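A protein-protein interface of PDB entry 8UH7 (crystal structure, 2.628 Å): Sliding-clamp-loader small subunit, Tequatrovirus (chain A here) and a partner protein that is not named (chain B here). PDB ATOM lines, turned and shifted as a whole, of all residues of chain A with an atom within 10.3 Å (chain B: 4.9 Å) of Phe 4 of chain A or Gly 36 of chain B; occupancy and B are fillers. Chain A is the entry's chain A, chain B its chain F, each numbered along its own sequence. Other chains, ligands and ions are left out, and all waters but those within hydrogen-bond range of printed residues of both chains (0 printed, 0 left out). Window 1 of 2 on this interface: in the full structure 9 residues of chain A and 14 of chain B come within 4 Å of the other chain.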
ATOM      1  N   SER A   2       6.299   1.915  11.987  1.00  0.00           N
ATOM      2  CA  SER A   2       6.210   0.650  11.266  1.00  0.00           C
ATOM      3  C   SER A   2       7.539  -0.099  11.296  1.00  0.00           C
ATOM      4  O   SER A   2       8.346   0.032  10.376  1.00  0.00           O
ATOM      5  CB  SER A   2       5.781   0.887   9.816  1.00  0.00           C
ATOM      6  OG  SER A   2       6.850   1.414   9.048  1.00  0.00           O
ATOM      7  N   LEU A   3       7.756  -0.883  12.358  1.00  0.00           N
ATOM      8  CA  LEU A   3       8.982  -1.667  12.476  1.00  0.00           C
ATOM      9  C   LEU A   3       9.196  -2.544  11.249  1.00  0.00           C
ATOM     10  O   LEU A   3      10.306  -2.635  10.716  1.00  0.00           O
ATOM     11  CB  LEU A   3       8.932  -2.523  13.743  1.00  0.00           C
ATOM     12  CG  LEU A   3       8.794  -1.753  15.056  1.00  0.00           C
ATOM     13  CD1 LEU A   3       8.552  -2.702  16.218  1.00  0.00           C
ATOM     14  CD2 LEU A   3      10.035  -0.917  15.296  1.00  0.00           C
ATOM     15  N   PHE A   4       8.132  -3.189  10.786  1.00  0.00           N
ATOM     16  CA  PHE A   4       8.165  -4.040   9.601  1.00  0.00           C
ATOM     17  C   PHE A   4       8.261  -3.148   8.371  1.00  0.00           C
ATOM     18  O   PHE A   4       7.263  -2.593   7.910  1.00  0.00           O
ATOM     19  CB  PHE A   4       6.920  -4.918   9.553  1.00  0.00           C
ATOM     20  CG  PHE A   4       6.484  -5.418  10.901  1.00  0.00           C
ATOM     21  CD1 PHE A   4       5.695  -4.630  11.730  1.00  0.00           C
ATOM     22  CD2 PHE A   4       6.866  -6.672  11.345  1.00  0.00           C
ATOM     23  CE1 PHE A   4       5.303  -5.081  12.970  1.00  0.00           C
ATOM     24  CE2 PHE A   4       6.472  -7.131  12.585  1.00  0.00           C
ATOM     25  CZ  PHE A   4       5.691  -6.335  13.398  1.00  0.00           C
ATOM     26  N   LYS A   5       9.471  -3.005   7.831  1.00  0.00           N
ATOM     27  CA  LYS A   5       9.715  -2.090   6.721  1.00  0.00           C
ATOM     28  C   LYS A   5       9.260  -2.643   5.375  1.00  0.00           C
ATOM     29  O   LYS A   5       9.552  -2.030   4.343  1.00  0.00           O
ATOM     30  CB  LYS A   5      11.200  -1.722   6.656  1.00  0.00           C
ATOM     31  CG  LYS A   5      11.694  -0.942   7.863  1.00  0.00           C
ATOM     32  CD  LYS A   5      12.867  -0.041   7.504  1.00  0.00           C
ATOM     33  CE  LYS A   5      12.459   1.018   6.489  1.00  0.00           C
ATOM     34  NZ  LYS A   5      13.460   2.115   6.376  1.00  0.00           N
ATOM     35  N   ASP A   6       8.567  -3.782   5.366  1.00  0.00           N
ATOM     36  CA  ASP A   6       8.003  -4.344   4.146  1.00  0.00           C
ATOM     37  C   ASP A   6       6.570  -3.848   3.980  1.00  0.00           C
ATOM     38  O   ASP A   6       6.325  -2.634   4.009  1.00  0.00           O
ATOM     39  CB  ASP A   6       8.056  -5.877   4.188  1.00  0.00           C
ATOM     40  CG  ASP A   6       9.327  -6.445   3.559  1.00  0.00           C
ATOM     41  OD1 ASP A   6       9.831  -5.868   2.570  1.00  0.00           O
ATOM     42  OD2 ASP A   6       9.809  -7.490   4.046  1.00  0.00           O
ATOM     43  N   ASP A   7       5.629  -4.785   3.802  1.00  0.00           N
ATOM     44  CA  ASP A   7       4.189  -4.529   3.798  1.00  0.00           C
ATOM     45  C   ASP A   7       3.738  -3.763   2.559  1.00  0.00           C
ATOM     46  O   ASP A   7       4.326  -2.740   2.195  1.00  0.00           O
ATOM     47  CB  ASP A   7       3.767  -3.785   5.069  1.00  0.00           C
ATOM     48  CG  ASP A   7       4.268  -4.464   6.330  1.00  0.00           C
ATOM     49  OD1 ASP A   7       4.752  -5.614   6.232  1.00  0.00           O
ATOM     50  OD2 ASP A   7       4.189  -3.848   7.412  1.00  0.00           O
ATOM     51  N   ILE A   8       2.698  -4.271   1.890  1.00  0.00           N
ATOM     52  CA  ILE A   8       2.049  -3.507   0.833  1.00  0.00           C
ATOM     53  C   ILE A   8       1.294  -2.323   1.420  1.00  0.00           C
ATOM     54  O   ILE A   8       0.930  -1.396   0.686  1.00  0.00           O
ATOM     55  CB  ILE A   8       1.110  -4.410   0.009  1.00  0.00           C
ATOM     56  CG1 ILE A   8       1.711  -5.810  -0.134  1.00  0.00           C
ATOM     57  CG2 ILE A   8       0.865  -3.815  -1.371  1.00  0.00           C
ATOM     58  CD1 ILE A   8       0.830  -6.781  -0.890  1.00  0.00           C
ATOM     59  N   GLN A   9       1.059  -2.339   2.736  1.00  0.00           N
ATOM     60  CA  GLN A   9       0.412  -1.269   3.490  1.00  0.00           C
ATOM     61  C   GLN A   9      -1.064  -1.137   3.136  1.00  0.00           C
ATOM     62  O   GLN A   9      -1.442  -1.147   1.960  1.00  0.00           O
ATOM     63  CB  GLN A   9       1.141   0.064   3.286  1.00  0.00           C
ATOM     64  CG  GLN A   9       2.100   0.417   4.414  1.00  0.00           C
ATOM     65  CD  GLN A   9       1.377   0.774   5.701  1.00  0.00           C
ATOM     66  OE1 GLN A   9       0.493   1.630   5.712  1.00  0.00           O
ATOM     67  NE2 GLN A   9       1.748   0.111   6.793  1.00  0.00           N
ATOM     68  N   LEU A  10      -1.900  -1.013   4.159  1.00  0.00           N
ATOM     69  CA  LEU A  10      -3.342  -0.937   4.003  1.00  0.00           C
ATOM     70  C   LEU A  10      -3.797   0.517   3.932  1.00  0.00           C
ATOM     71  O   LEU A  10      -3.084   1.439   4.332  1.00  0.00           O
ATOM     72  CB  LEU A  10      -4.033  -1.642   5.169  1.00  0.00           C
ATOM     73  CG  LEU A  10      -3.416  -2.966   5.622  1.00  0.00           C
ATOM     74  CD1 LEU A  10      -4.109  -3.486   6.871  1.00  0.00           C
ATOM     75  CD2 LEU A  10      -3.479  -3.992   4.504  1.00  0.00           C
ATOM     76  N   VAL A  15      -6.917  -0.094   8.309  1.00  0.00           N
ATOM     77  CA  VAL A  15      -6.224   0.120   9.576  1.00  0.00           C
ATOM     78  C   VAL A  15      -7.224   0.431  10.680  1.00  0.00           C
ATOM     79  O   VAL A  15      -7.070  -0.018  11.822  1.00  0.00           O
ATOM     80  CB  VAL A  15      -5.172   1.235   9.429  1.00  0.00           C
ATOM     81  CG1 VAL A  15      -4.460   1.479  10.752  1.00  0.00           C
ATOM     82  CG2 VAL A  15      -4.172   0.879   8.342  1.00  0.00           C
ATOM     83  N   SER A  19      -7.881  -2.833  13.402  1.00  0.00           N
ATOM     84  CA  SER A  19      -7.483  -2.463  14.755  1.00  0.00           C
ATOM     85  C   SER A  19      -8.670  -2.325  15.693  1.00  0.00           C
ATOM     86  O   SER A  19      -8.480  -2.337  16.915  1.00  0.00           O
ATOM     87  CB  SER A  19      -6.695  -1.153  14.740  1.00  0.00           C
ATOM     88  OG  SER A  19      -7.451  -0.104  14.161  1.00  0.00           O
ATOM     89  N   ARG B  32       1.539  -8.100  16.366  1.00  0.00           N
ATOM     90  CA  ARG B  32       1.945  -6.790  15.891  1.00  0.00           C
ATOM     91  C   ARG B  32       0.752  -5.850  15.929  1.00  0.00           C
ATOM     92  O   ARG B  32      -0.400  -6.277  15.811  1.00  0.00           O
ATOM     93  CB  ARG B  32       2.508  -6.840  14.465  1.00  0.00           C
ATOM     94  CG  ARG B  32       1.470  -7.101  13.389  1.00  0.00           C
ATOM     95  CD  ARG B  32       2.033  -6.863  11.997  1.00  0.00           C
ATOM     96  NE  ARG B  32       2.115  -5.441  11.676  1.00  0.00           N
ATOM     97  CZ  ARG B  32       2.579  -4.959  10.528  1.00  0.00           C
ATOM     98  NH1 ARG B  32       3.013  -5.785   9.584  1.00  0.00           N
ATOM     99  NH2 ARG B  32       2.615  -3.648  10.322  1.00  0.00           N
ATOM    100  N   ALA B  33       1.038  -4.566  16.107  1.00  0.00           N
ATOM    101  CA  ALA B  33       0.003  -3.568  15.924  1.00  0.00           C
ATOM    102  C   ALA B  33      -0.338  -3.449  14.444  1.00  0.00           C
ATOM    103  O   ALA B  33       0.447  -3.818  13.565  1.00  0.00           O
ATOM    104  CB  ALA B  33       0.451  -2.217  16.474  1.00  0.00           C
ATOM    105  N   VAL B  34      -1.536  -2.931  14.170  1.00  0.00           N
ATOM    106  CA  VAL B  34      -1.960  -2.793  12.783  1.00  0.00           C
ATOM    107  C   VAL B  34      -1.127  -1.735  12.074  1.00  0.00           C
ATOM    108  O   VAL B  34      -0.822  -1.872  10.882  1.00  0.00           O
ATOM    109  CB  VAL B  34      -3.465  -2.482  12.719  1.00  0.00           C
ATOM    110  CG1 VAL B  34      -3.980  -2.635  11.298  1.00  0.00           C
ATOM    111  CG2 VAL B  34      -4.220  -3.395  13.666  1.00  0.00           C
ATOM    112  N   ASN B  35      -0.729  -0.679  12.783  1.00  0.00           N
ATOM    113  CA  ASN B  35       0.147   0.348  12.234  1.00  0.00           C
ATOM    114  C   ASN B  35       1.624   0.002  12.386  1.00  0.00           C
ATOM    115  O   ASN B  35       2.478   0.834  12.061  1.00  0.00           O
ATOM    116  CB  ASN B  35      -0.141   1.701  12.888  1.00  0.00           C
ATOM    117  CG  ASN B  35      -0.003   1.657  14.393  1.00  0.00           C
ATOM    118  OD1 ASN B  35      -0.078   0.589  14.999  1.00  0.00           O
ATOM    119  ND2 ASN B  35       0.191   2.818  15.006  1.00  0.00           N
ATOM    120  N   GLY B  36       1.938  -1.193  12.884  1.00  0.00           N
ATOM    121  CA  GLY B  36       3.303  -1.682  12.924  1.00  0.00           C
ATOM    122  C   GLY B  36       4.225  -0.932  13.866  1.00  0.00           C
ATOM    123  O   GLY B  36       5.440  -1.146  13.845  1.00  0.00           O
ATOM    124  N   THR B  37       3.664  -0.058  14.705  1.00  0.00           N
ATOM    125  CA  THR B  37       4.500   0.771  15.567  1.00  0.00           C
ATOM    126  C   THR B  37       4.989   0.026  16.805  1.00  0.00           C
ATOM    127  O   THR B  37       6.043   0.373  17.347  1.00  0.00           O
ATOM    128  CB  THR B  37       3.746   2.034  15.984  1.00  0.00           C
ATOM    129  OG1 THR B  37       2.480   1.677  16.550  1.00  0.00           O
ATOM    130  CG2 THR B  37       3.533   2.951  14.786  1.00  0.00           C
ATOM    131  N   THR B  38       4.258  -0.987  17.267  1.00  0.00           N
ATOM    132  CA  THR B  38       4.692  -1.797  18.395  1.00  0.00           C
ATOM    133  C   THR B  38       4.625  -3.274  18.028  1.00  0.00           C
ATOM    134  O   THR B  38       3.965  -3.668  17.063  1.00  0.00           O
ATOM    135  CB  THR B  38       3.858  -1.521  19.659  1.00  0.00           C
ATOM    136  OG1 THR B  38       4.084  -2.558  20.624  1.00  0.00           O
ATOM    137  CG2 THR B  38       2.380  -1.451  19.331  1.00  0.00           C
ATOM    138  N   TYR B  39       5.327  -4.089  18.816  1.00  0.00           N
ATOM    139  CA  TYR B  39       5.484  -5.508  18.535  1.00  0.00           C
ATOM    140  C   TYR B  39       5.749  -6.247  19.840  1.00  0.00           C
ATOM    141  O   TYR B  39       6.340  -5.694  20.770  1.00  0.00           O
ATOM    142  CB  TYR B  39       6.626  -5.738  17.534  1.00  0.00           C
ATOM    143  CG  TYR B  39       7.183  -7.144  17.506  1.00  0.00           C
ATOM    144  CD1 TYR B  39       8.229  -7.515  18.344  1.00  0.00           C
ATOM    145  CD2 TYR B  39       6.677  -8.093  16.634  1.00  0.00           C
ATOM    146  CE1 TYR B  39       8.742  -8.795  18.322  1.00  0.00           C
ATOM    147  CE2 TYR B  39       7.186  -9.373  16.603  1.00  0.00           C
ATOM    148  CZ  TYR B  39       8.218  -9.719  17.448  1.00  0.00           C
ATOM    149  OH  TYR B  39       8.729 -10.997  17.419  1.00  0.00           O
ATOM    150  N   PRO B 103       2.560 -10.391  12.255  1.00  0.00           N
ATOM    151  CA  PRO B 103       3.936 -10.292  11.747  1.00  0.00           C
ATOM    152  C   PRO B 103       4.278 -11.506  10.899  1.00  0.00           C
ATOM    153  O   PRO B 103       4.169 -12.651  11.346  1.00  0.00           O
ATOM    154  CB  PRO B 103       4.780 -10.225  13.026  1.00  0.00           C
ATOM    155  CG  PRO B 103       3.912 -10.816  14.093  1.00  0.00           C
ATOM    156  CD  PRO B 103       2.509 -10.476  13.725  1.00  0.00           C
ATOM    157  N   ASN B 104       4.685 -11.249   9.653  1.00  0.00           N
ATOM    158  CA  ASN B 104       4.945 -12.333   8.711  1.00  0.00           C
ATOM    159  C   ASN B 104       6.101 -13.224   9.153  1.00  0.00           C
ATOM    160  O   ASN B 104       6.208 -14.359   8.674  1.00  0.00           O
ATOM    161  CB  ASN B 104       5.219 -11.765   7.315  1.00  0.00           C
ATOM    162  CG  ASN B 104       6.459 -10.885   7.267  1.00  0.00           C
ATOM    163  OD1 ASN B 104       6.776 -10.180   8.227  1.00  0.00           O
ATOM    164  ND2 ASN B 104       7.166 -10.924   6.144  1.00  0.00           N
ATOM    165  N   ILE B 107      10.859 -10.830  14.130  1.00  0.00           N
ATOM    166  CA  ILE B 107      11.699  -9.723  13.659  1.00  0.00           C
ATOM    167  C   ILE B 107      13.142  -9.962  14.090  1.00  0.00           C
ATOM    168  O   ILE B 107      13.377 -10.438  15.215  1.00  0.00           O
ATOM    169  CB  ILE B 107      11.171  -8.390  14.183  1.00  0.00           C
ATOM    170  CG1 ILE B 107      11.221  -8.350  15.711  1.00  0.00           C
ATOM    171  CG2 ILE B 107       9.741  -8.165  13.701  1.00  0.00           C
ATOM    172  CD1 ILE B 107      11.032  -6.979  16.282  1.00  0.00           C
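Of the printed residues of chain B, Ser 2 of chain A touches Asn 35 and Gly 36. Of chain B, only Arg 32 (3.4 Å), Gly 36 (3.9 Å), Tyr 39 (3.8 Å), Pro 103 (3.6 Å) and Ile 107 (3.6 Å) come within 4 Å of Phe 4 of chain A. Of the printed residues of chain B, Val 15 of chain A touches Val 34 (3.9 Å). Of chain A, only Ser 2 (3.2 Å), Leu 3 (2.8 Å) and Phe 4 (3.9 Å) come within 4 Å of Gly 36 of chain B. No residue of chain A comes within 4 Å of Thr 37 of chain B. The nearest residue of chain A that does not touch Gly 36 of chain B is Asp 7 of chain A (6.0 Å). The nearest printed residue of chain A that does not touch Ile 107 of chain B is Leu 3 of chain A (4.9 Å).
Of the 11 printed residues of chain B, 7 touch a printed residue of chain A. Hydrophobic or aromatic side chains of chain B that line the printed part of chain A: Val 34, Tyr 39, Pro 103 and Ile 107. Printed residues of chain A that touch a printed residue of chain B: Ser 2, Leu 3, Phe 4, Asp 7, Val 15 and Ser 19. Among the printed residues, 12 pairs touch across the chains. Among the printed residues, Asp or Glu carboxylates within 4 Å of a Lys or Arg side-chain nitrogen of the other chain: Asp 7 of chain A with Arg 32 of chain B (3.1 Å).
ND2 of Asn 35 of chain B sits at hydrogen-bond distance from OG1 of Thr 37 of chain B, 3.0 Å away.
Ser 2 of chain A touches Asn 35 of chain B (CA to O, 3.8 Å). CA of Ser 2 of chain A touches O of Gly 36 of chain B, at 3.2 Å. Leu 3 of chain A touches Tyr 39 of chain B. CZ of Arg 32 of chain B touches CD1 of Phe 4 of chain A, 3.4 Å away. Phe 4 of chain A touches Gly 36 of chain B (CE1 to CA, 3.9 Å). Tyr 39 of chain B touches Phe 4 of chain A (CD2 to CZ, 3.8 Å). Pro 103 of chain B touches Phe 4 of chain A. CE2 of Phe 4 of chain A touches CG2 of Ile 107 of chain B (3.6 Å). Val 15 of chain A touches Val 34 of chain B. Val 34 of chain B touches Ser 19 of chain A.
N of Leu 3 of chain A sits at hydrogen-bond distance from O of Gly 36 of chain B (2.8 Å). The side-chain carboxylate (OD2) of Asp 7 of chain A is in salt-bridge range of the guanidinium group (NH1) of Arg 32 of chain B (3.1 Å).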
